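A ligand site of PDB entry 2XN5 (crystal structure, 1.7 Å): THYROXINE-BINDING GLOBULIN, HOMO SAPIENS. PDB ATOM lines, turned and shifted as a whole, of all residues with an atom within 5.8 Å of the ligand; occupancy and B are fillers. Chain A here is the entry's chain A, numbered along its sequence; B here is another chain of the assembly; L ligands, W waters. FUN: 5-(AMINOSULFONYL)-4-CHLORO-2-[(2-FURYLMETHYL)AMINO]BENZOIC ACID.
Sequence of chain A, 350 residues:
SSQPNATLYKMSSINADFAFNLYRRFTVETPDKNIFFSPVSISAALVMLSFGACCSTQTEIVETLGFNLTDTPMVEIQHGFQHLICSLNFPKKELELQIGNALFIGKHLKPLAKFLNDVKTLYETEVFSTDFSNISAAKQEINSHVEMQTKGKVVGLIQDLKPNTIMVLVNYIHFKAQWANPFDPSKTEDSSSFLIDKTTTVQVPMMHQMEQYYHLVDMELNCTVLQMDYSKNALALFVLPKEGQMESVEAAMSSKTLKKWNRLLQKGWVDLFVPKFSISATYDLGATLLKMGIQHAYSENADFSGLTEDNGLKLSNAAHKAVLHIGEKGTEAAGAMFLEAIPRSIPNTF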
ATOM      1  N   TYR A   9     -13.665   9.911 -23.712  1.00  0.00           N
ATOM      2  CA  TYR A   9     -12.772   9.752 -22.557  1.00  0.00           C
ATOM      3  C   TYR A   9     -12.508  11.077 -21.829  1.00  0.00           C
ATOM      4  O   TYR A   9     -12.314  11.072 -20.614  1.00  0.00           O
ATOM      5  CB  TYR A   9     -11.442   9.079 -22.933  1.00  0.00           C
ATOM      6  CG  TYR A   9     -11.580   7.725 -23.594  1.00  0.00           C
ATOM      7  CD1 TYR A   9     -12.548   6.800 -23.180  1.00  0.00           C
ATOM      8  CD2 TYR A   9     -10.728   7.355 -24.633  1.00  0.00           C
ATOM      9  CE1 TYR A   9     -12.663   5.563 -23.796  1.00  0.00           C
ATOM     10  CE2 TYR A   9     -10.836   6.113 -25.253  1.00  0.00           C
ATOM     11  CZ  TYR A   9     -11.804   5.234 -24.837  1.00  0.00           C
ATOM     12  OH  TYR A   9     -11.912   4.009 -25.460  1.00  0.00           O
ATOM     13  N   SER A  12     -15.513  11.690 -19.588  1.00  0.00           N
ATOM     14  CA  SER A  12     -15.533  10.822 -18.416  1.00  0.00           C
ATOM     15  C   SER A  12     -14.483  11.215 -17.379  1.00  0.00           C
ATOM     16  O   SER A  12     -14.729  11.089 -16.174  1.00  0.00           O
ATOM     17  CB  SER A  12     -15.373   9.344 -18.804  1.00  0.00           C
ATOM     18  OG  SER A  12     -14.073   9.058 -19.284  1.00  0.00           O
ATOM     19  N   SER A  13     -13.332  11.711 -17.840  1.00  0.00           N
ATOM     20  CA  SER A  13     -12.256  12.177 -16.940  1.00  0.00           C
ATOM     21  C   SER A  13     -12.668  13.472 -16.217  1.00  0.00           C
ATOM     22  O   SER A  13     -12.412  13.639 -15.026  1.00  0.00           O
ATOM     23  CB  SER A  13     -10.940  12.419 -17.686  1.00  0.00           C
ATOM     24  OG  SER A  13     -10.273  11.204 -18.013  1.00  0.00           O
ATOM     25  N   ALA A  16     -15.299  12.473 -13.786  1.00  0.00           N
ATOM     26  CA  ALA A  16     -14.750  11.780 -12.609  1.00  0.00           C
ATOM     27  C   ALA A  16     -14.164  12.776 -11.616  1.00  0.00           C
ATOM     28  O   ALA A  16     -14.295  12.623 -10.411  1.00  0.00           O
ATOM     29  CB  ALA A  16     -13.712  10.738 -13.035  1.00  0.00           C
ATOM     30  N   PHE A  20     -15.298  13.420  -7.638  1.00  0.00           N
ATOM     31  CA  PHE A  20     -14.465  13.490  -6.423  1.00  0.00           C
ATOM     32  C   PHE A  20     -14.550  14.846  -5.724  1.00  0.00           C
ATOM     33  O   PHE A  20     -14.490  14.904  -4.499  1.00  0.00           O
ATOM     34  CB  PHE A  20     -13.005  13.099  -6.722  1.00  0.00           C
ATOM     35  CG  PHE A  20     -12.833  11.631  -7.085  1.00  0.00           C
ATOM     36  CD1 PHE A  20     -13.164  10.627  -6.170  1.00  0.00           C
ATOM     37  CD2 PHE A  20     -12.370  11.269  -8.338  1.00  0.00           C
ATOM     38  CE1 PHE A  20     -13.005   9.282  -6.524  1.00  0.00           C
ATOM     39  CE2 PHE A  20     -12.217   9.948  -8.690  1.00  0.00           C
ATOM     40  CZ  PHE A  20     -12.526   8.950  -7.776  1.00  0.00           C
ATOM     41  N   GLN A 227     -10.125  -4.818  -6.685  1.00  0.00           N
ATOM     42  CA  GLN A 227     -11.075  -4.751  -7.787  1.00  0.00           C
ATOM     43  C   GLN A 227     -11.838  -6.056  -7.874  1.00  0.00           C
ATOM     44  O   GLN A 227     -11.233  -7.129  -7.902  1.00  0.00           O
ATOM     45  CB  GLN A 227     -10.330  -4.539  -9.099  1.00  0.00           C
ATOM     46  CG  GLN A 227     -11.193  -4.657 -10.356  1.00  0.00           C
ATOM     47  CD  GLN A 227     -10.418  -4.350 -11.625  1.00  0.00           C
ATOM     48  OE1 GLN A 227      -9.728  -3.339 -11.698  1.00  0.00           O
ATOM     49  NE2 GLN A 227     -10.518  -5.228 -12.628  1.00  0.00           N
ATOM     50  N   LEU A 235     -16.881  -2.996 -13.298  1.00  0.00           N
ATOM     51  CA  LEU A 235     -16.123  -3.430 -12.124  1.00  0.00           C
ATOM     52  C   LEU A 235     -16.403  -2.557 -10.912  1.00  0.00           C
ATOM     53  O   LEU A 235     -16.900  -1.436 -11.049  1.00  0.00           O
ATOM     54  CB  LEU A 235     -14.629  -3.438 -12.448  1.00  0.00           C
ATOM     55  CG  LEU A 235     -14.021  -2.079 -12.807  1.00  0.00           C
ATOM     56  CD1 LEU A 235     -13.523  -1.386 -11.523  1.00  0.00           C
ATOM     57  CD2 LEU A 235     -12.893  -2.255 -13.792  1.00  0.00           C
ATOM     58  N   LEU A 237     -14.440  -1.067  -7.396  1.00  0.00           N
ATOM     59  CA  LEU A 237     -13.189  -0.864  -6.683  1.00  0.00           C
ATOM     60  C   LEU A 237     -13.475  -0.574  -5.224  1.00  0.00           C
ATOM     61  O   LEU A 237     -14.281   0.299  -4.901  1.00  0.00           O
ATOM     62  CB  LEU A 237     -12.365   0.290  -7.275  1.00  0.00           C
ATOM     63  CG  LEU A 237     -11.904   0.185  -8.725  1.00  0.00           C
ATOM     64  CD1 LEU A 237     -11.324   1.503  -9.203  1.00  0.00           C
ATOM     65  CD2 LEU A 237     -10.889  -0.950  -8.911  1.00  0.00           C
ATOM     66  N   SER A 254      -8.694  11.586  -7.589  1.00  0.00           N
ATOM     67  CA  SER A 254      -8.953  12.316  -8.830  1.00  0.00           C
ATOM     68  C   SER A 254      -8.982  11.297  -9.962  1.00  0.00           C
ATOM     69  O   SER A 254      -8.703  10.096  -9.751  1.00  0.00           O
ATOM     70  CB  SER A 254      -7.870  13.372  -9.083  1.00  0.00           C
ATOM     71  OG  SER A 254      -6.611  12.764  -9.289  1.00  0.00           O
ATOM     72  N   SER A 255      -9.308  11.762 -11.169  1.00  0.00           N
ATOM     73  CA  SER A 255      -9.191  10.958 -12.376  1.00  0.00           C
ATOM     74  C   SER A 255      -7.762  10.438 -12.553  1.00  0.00           C
ATOM     75  O   SER A 255      -7.576   9.301 -13.010  1.00  0.00           O
ATOM     76  CB  SER A 255      -9.628  11.743 -13.615  1.00  0.00           C
ATOM     77  OG  SER A 255      -8.856  12.914 -13.802  1.00  0.00           O
ATOM     78  N   LYS A 256      -6.779  11.259 -12.172  1.00  0.00           N
ATOM     79  CA  LYS A 256      -5.355  10.910 -12.261  1.00  0.00           C
ATOM     80  C   LYS A 256      -5.046   9.667 -11.417  1.00  0.00           C
ATOM     81  O   LYS A 256      -4.242   8.827 -11.836  1.00  0.00           O
ATOM     82  CB  LYS A 256      -4.500  12.113 -11.844  1.00  0.00           C
ATOM     83  CG  LYS A 256      -2.998  12.001 -12.074  1.00  0.00           C
ATOM     84  CD  LYS A 256      -2.283  13.365 -11.937  1.00  0.00           C
ATOM     85  CE  LYS A 256      -0.814  13.206 -11.526  1.00  0.00           C
ATOM     86  NZ  LYS A 256      -0.131  14.510 -11.278  1.00  0.00           N
ATOM     87  N   LEU A 258      -7.210   7.198 -10.753  1.00  0.00           N
ATOM     88  CA  LEU A 258      -7.788   6.049 -11.440  1.00  0.00           C
ATOM     89  C   LEU A 258      -6.921   5.649 -12.644  1.00  0.00           C
ATOM     90  O   LEU A 258      -6.730   4.459 -12.901  1.00  0.00           O
ATOM     91  CB  LEU A 258      -9.242   6.335 -11.856  1.00  0.00           C
ATOM     92  CG  LEU A 258     -10.202   6.652 -10.690  1.00  0.00           C
ATOM     93  CD1 LEU A 258     -11.660   6.563 -11.115  1.00  0.00           C
ATOM     94  CD2 LEU A 258      -9.978   5.748  -9.475  1.00  0.00           C
ATOM     95  N   LYS A 259      -6.384   6.628 -13.357  1.00  0.00           N
ATOM     96  CA  LYS A 259      -5.463   6.355 -14.459  1.00  0.00           C
ATOM     97  C   LYS A 259      -4.194   5.632 -13.976  1.00  0.00           C
ATOM     98  O   LYS A 259      -3.694   4.746 -14.663  1.00  0.00           O
ATOM     99  CB  LYS A 259      -5.123   7.647 -15.205  1.00  0.00           C
ATOM    100  CG  LYS A 259      -6.313   8.219 -15.973  1.00  0.00           C
ATOM    101  CD  LYS A 259      -5.989   9.515 -16.726  1.00  0.00           C
ATOM    102  CE  LYS A 259      -7.233  10.142 -17.354  1.00  0.00           C
ATOM    103  NZ  LYS A 259      -6.949  11.475 -17.967  1.00  0.00           N
ATOM    104  N   TRP A 261      -3.977   3.753 -11.090  1.00  0.00           N
ATOM    105  CA  TRP A 261      -4.376   2.417 -10.641  1.00  0.00           C
ATOM    106  C   TRP A 261      -4.644   1.479 -11.828  1.00  0.00           C
ATOM    107  O   TRP A 261      -4.356   0.272 -11.735  1.00  0.00           O
ATOM    108  CB  TRP A 261      -5.591   2.456  -9.700  1.00  0.00           C
ATOM    109  CG  TRP A 261      -5.323   3.099  -8.335  1.00  0.00           C
ATOM    110  CD1 TRP A 261      -4.106   3.389  -7.776  1.00  0.00           C
ATOM    111  CD2 TRP A 261      -6.309   3.509  -7.367  1.00  0.00           C
ATOM    112  NE1 TRP A 261      -4.264   3.964  -6.545  1.00  0.00           N
ATOM    113  CE2 TRP A 261      -5.606   4.040  -6.257  1.00  0.00           C
ATOM    114  CE3 TRP A 261      -7.703   3.488  -7.336  1.00  0.00           C
ATOM    115  CZ2 TRP A 261      -6.255   4.555  -5.133  1.00  0.00           C
ATOM    116  CZ3 TRP A 261      -8.345   3.992  -6.208  1.00  0.00           C
ATOM    117  CH2 TRP A 261      -7.616   4.515  -5.118  1.00  0.00           C
ATOM    118  N   ASN A 262      -5.186   2.010 -12.919  1.00  0.00           N
ATOM    119  CA  ASN A 262      -5.386   1.205 -14.130  1.00  0.00           C
ATOM    120  C   ASN A 262      -4.090   0.515 -14.577  1.00  0.00           C
ATOM    121  O   ASN A 262      -4.101  -0.646 -15.013  1.00  0.00           O
ATOM    122  CB  ASN A 262      -5.932   2.086 -15.256  1.00  0.00           C
ATOM    123  CG  ASN A 262      -6.132   1.309 -16.554  1.00  0.00           C
ATOM    124  OD1 ASN A 262      -7.028   0.468 -16.642  1.00  0.00           O
ATOM    125  ND2 ASN A 262      -5.305   1.597 -17.557  1.00  0.00           N
ATOM    126  N   LEU A 265      -2.612  -1.948 -11.055  1.00  0.00           N
ATOM    127  CA  LEU A 265      -3.378  -3.106 -10.578  1.00  0.00           C
ATOM    128  C   LEU A 265      -2.858  -4.398 -11.216  1.00  0.00           C
ATOM    129  O   LEU A 265      -2.657  -4.455 -12.427  1.00  0.00           O
ATOM    130  CB  LEU A 265      -4.867  -2.935 -10.899  1.00  0.00           C
ATOM    131  CG  LEU A 265      -5.618  -1.966  -9.968  1.00  0.00           C
ATOM    132  CD1 LEU A 265      -6.939  -1.560 -10.617  1.00  0.00           C
ATOM    133  CD2 LEU A 265      -5.853  -2.604  -8.596  1.00  0.00           C
ATOM    134  N   LEU B  16     -17.457   1.330 -11.818  1.00  0.00           N
ATOM    135  CA  LEU B  16     -17.140   1.949 -13.088  1.00  0.00           C
ATOM    136  C   LEU B  16     -17.479   1.081 -14.273  1.00  0.00           C
ATOM    137  O   LEU B  16     -17.548  -0.165 -14.163  1.00  0.00           O
ATOM    138  CB  LEU B  16     -15.693   2.467 -13.122  1.00  0.00           C
ATOM    139  CG  LEU B  16     -14.454   1.604 -13.308  1.00  0.00           C
ATOM    140  CD1 LEU B  16     -14.078   1.499 -14.790  1.00  0.00           C
ATOM    141  CD2 LEU B  16     -13.260   2.173 -12.477  1.00  0.00           C
ATOM    142  N   ARG B  18     -16.315   0.156 -18.025  1.00  0.00           N
ATOM    143  CA  ARG B  18     -14.975   0.193 -18.619  1.00  0.00           C
ATOM    144  C   ARG B  18     -14.912   0.862 -19.990  1.00  0.00           C
ATOM    145  O   ARG B  18     -13.977   1.622 -20.257  1.00  0.00           O
ATOM    146  CB  ARG B  18     -14.330  -1.202 -18.693  1.00  0.00           C
ATOM    147  CG  ARG B  18     -12.808  -1.139 -18.895  1.00  0.00           C
ATOM    148  CD  ARG B  18     -12.177  -2.511 -19.092  1.00  0.00           C
ATOM    149  NE  ARG B  18     -12.113  -3.291 -17.855  1.00  0.00           N
ATOM    150  CZ  ARG B  18     -11.164  -3.191 -16.929  1.00  0.00           C
ATOM    151  NH1 ARG B  18     -11.229  -3.974 -15.854  1.00  0.00           N
ATOM    152  NH2 ARG B  18     -10.160  -2.321 -17.048  1.00  0.00           N
ATOM    153  N   THR B  20     -16.562   3.249 -21.465  1.00  0.00           N
ATOM    154  CA  THR B  20     -16.613   4.715 -21.407  1.00  0.00           C
ATOM    155  C   THR B  20     -15.718   5.277 -20.314  1.00  0.00           C
ATOM    156  O   THR B  20     -15.548   6.503 -20.247  1.00  0.00           O
ATOM    157  CB  THR B  20     -18.046   5.221 -21.122  1.00  0.00           C
ATOM    158  OG1 THR B  20     -18.436   4.861 -19.786  1.00  0.00           O
ATOM    159  CG2 THR B  20     -19.039   4.620 -22.117  1.00  0.00           C
ATOM    160  N   ARG B  21     -15.203   4.403 -19.452  1.00  0.00           N
ATOM    161  CA  ARG B  21     -14.402   4.777 -18.268  1.00  0.00           C
ATOM    162  C   ARG B  21     -15.159   5.718 -17.328  1.00  0.00           C
ATOM    163  O   ARG B  21     -14.582   6.623 -16.721  1.00  0.00           O
ATOM    164  CB  ARG B  21     -13.048   5.365 -18.683  1.00  0.00           C
ATOM    165  CG  ARG B  21     -12.209   4.406 -19.522  1.00  0.00           C
ATOM    166  CD  ARG B  21     -11.049   5.116 -20.193  1.00  0.00           C
ATOM    167  NE  ARG B  21     -10.478   4.294 -21.258  1.00  0.00           N
ATOM    168  CZ  ARG B  21      -9.479   4.679 -22.057  1.00  0.00           C
ATOM    169  NH1 ARG B  21      -8.930   5.876 -21.921  1.00  0.00           N
ATOM    170  NH2 ARG B  21      -9.036   3.861 -22.996  1.00  0.00           N
ATOM    171  N   SER B  22     -16.464   5.476 -17.187  1.00  0.00           N
ATOM    172  CA  SER B  22     -17.356   6.322 -16.397  1.00  0.00           C
ATOM    173  C   SER B  22     -17.517   5.804 -14.977  1.00  0.00           C
ATOM    174  O   SER B  22     -17.720   4.610 -14.772  1.00  0.00           O
ATOM    175  CB  SER B  22     -18.733   6.403 -17.068  1.00  0.00           C
ATOM    176  OG  SER B  22     -19.656   7.165 -16.293  1.00  0.00           O
ATOM    177  N   ILE B  23     -17.459   6.711 -14.009  1.00  0.00           N
ATOM    178  CA  ILE B  23     -17.821   6.386 -12.637  1.00  0.00           C
ATOM    179  C   ILE B  23     -19.350   6.486 -12.522  1.00  0.00           C
ATOM    180  O   ILE B  23     -19.909   7.591 -12.519  1.00  0.00           O
ATOM    181  CB  ILE B  23     -17.188   7.351 -11.622  1.00  0.00           C
ATOM    182  CG1 ILE B  23     -15.670   7.369 -11.766  1.00  0.00           C
ATOM    183  CG2 ILE B  23     -17.599   6.957 -10.198  1.00  0.00           C
ATOM    184  CD1 ILE B  23     -14.988   8.293 -10.803  1.00  0.00           C
HETATM  185  N1  FUN L   1     -12.436   8.603 -16.257  1.00  0.00           N
HETATM  186  S1  FUN L   1     -11.191   8.332 -15.389  1.00  0.00           S
HETATM  187  O1  FUN L   1     -10.149   9.255 -15.875  1.00  0.00           O
HETATM  188  O2  FUN L   1     -11.528   8.539 -13.976  1.00  0.00           O
HETATM  189  C1  FUN L   1     -10.737   6.792 -15.644  1.00  0.00           C
HETATM  190  C2  FUN L   1     -11.407   5.714 -15.074  1.00  0.00           C
HETATM  191 CL1  FUN L   1     -12.846   5.894 -14.022  1.00  0.00          CL
HETATM  192  C3  FUN L   1     -11.008   4.405 -15.290  1.00  0.00           C
HETATM  193  C4  FUN L   1      -9.909   4.114 -16.103  1.00  0.00           C
HETATM  194  N2  FUN L   1      -9.525   2.822 -16.319  1.00  0.00           N
HETATM  195  C5  FUN L   1     -10.230   1.651 -15.825  1.00  0.00           C
HETATM  196  C6  FUN L   1      -9.826   1.269 -14.418  1.00  0.00           C
HETATM  197  C7  FUN L   1      -9.131   2.046 -13.499  1.00  0.00           C
HETATM  198  C8  FUN L   1      -8.988   1.307 -12.345  1.00  0.00           C
HETATM  199  C9  FUN L   1      -9.577   0.082 -12.546  1.00  0.00           C
HETATM  200  O3  FUN L   1     -10.099   0.072 -13.828  1.00  0.00           O
HETATM  201  C10 FUN L   1      -9.212   5.179 -16.684  1.00  0.00           C
HETATM  202  C11 FUN L   1      -9.640   6.498 -16.434  1.00  0.00           C
HETATM  203  C12 FUN L   1      -8.027   4.974 -17.591  1.00  0.00           C
HETATM  204  O4  FUN L   1      -7.581   5.931 -18.289  1.00  0.00           O
HETATM  205  O5  FUN L   1      -7.551   3.824 -17.694  1.00  0.00           O
HETATM  206  O   HOH W   1      -6.405   3.442 -20.402  1.00  0.00           O
HETATM  207  O   HOH W   2      -5.282   6.078 -19.362  1.00  0.00           O
HETATM  208  O   HOH W   3      -9.019   7.848 -19.847  1.00  0.00           O
HETATM  209  O   HOH W   4     -11.574   8.862 -19.100  1.00  0.00           O
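Ala 16 of chain A touches the ligand (CB to O2, 3.2 Å).
Gln 227 touches the ligand (OE1 to C9, 3.5 Å).
Leu 235 touches the ligand.
Leu 237 touches the ligand (CD1 to C8, 3.9 Å).
CB of Ser 255 touches O1 of the ligand, 3.4 Å away.
Leu 258 touches the ligand.
Lys 259 touches the ligand (CE to O1, 3.4 Å).
Leu 265 touches the ligand (CD1 to C9, 3.7 Å).
Leu 16 of chain B touches the ligand.
Ile 23 of chain B touches the ligand.
Hydrophobic or aromatic side chains within 4 Å of the ligand: Ala 16 of chain A, Leu 235, Leu 237, Leu 258, Leu 265, Leu 16 of chain B and Ile 23 of chain B.
14 residues have an atom within 4 Å of the ligand: Ser 12, Ser 13, Ala 16 of chain A, Gln 227, Leu 235, Leu 237, Ser 255, Leu 258, Lys 259, Asn 262, Leu 265, Leu 16 of chain B, Arg 21 of chain B and Ile 23 of chain B.
The nearest printed residue that does not touch the ligand is Arg 18 of chain B (4.01 Å).
Water W3 lies within hydrogen-bond range of O4 of the ligand (2.9 Å) and NH1 of Arg 21 of chain B (2.9 Å).
Water W4 lies within hydrogen-bond range of OG of Ser 12 (2.5 Å), O of Tyr 9 (2.8 Å), OG of Ser 13 (2.9 Å) and N1 of the ligand (3.0 Å).
The side-chain hydroxyl (OG) of Ser 13 lies within hydrogen-bond range of an oxygen (O1) of the ligand, at 2.9 Å.
The backbone carbonyl oxygen (O) of Arg 21 of chain B lies within hydrogen-bond range of a nitrogen (N1) of the ligand (3.0 Å).
The guanidinium group (NH1) of Arg 21 of chain B lies within salt-bridge range of an oxygen (O4) of the ligand, 3.9 Å away.
The side-chain amide nitrogen (ND2) of Asn 262 lies close to an oxygen (O5) of the ligand (3.2 Å).
The backbone carbonyl oxygen of Ser 12 is in hydrogen-bond range of a nitrogen (N1) of the ligand, at 3.4 Å.
The side-chain hydroxyl (OG) of Ser 12 lies within hydrogen-bond range of a nitrogen (N1) of the ligand, at 3.5 Å.
The side-chain amino group (NZ) of Lys 259 sits close to the side-chain hydroxyl (OG) of Ser 13, 3.3 Å away.
The backbone carbonyl oxygen (O) of Tyr 9 sits at hydrogen-bond distance from the side-chain hydroxyl (OG) of Ser 13, at 3.3 Å.
OG of Ser 12 is in hydrogen-bond range of O of Tyr 9.
OG of Ser 12 lies within hydrogen-bond range of O of Thr 20 of chain B (3.1 Å).
The backbone carbonyl oxygen (O) of Leu 235 lies within hydrogen-bond range of the backbone NH (N) of Leu 16 of chain B (2.9 Å).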
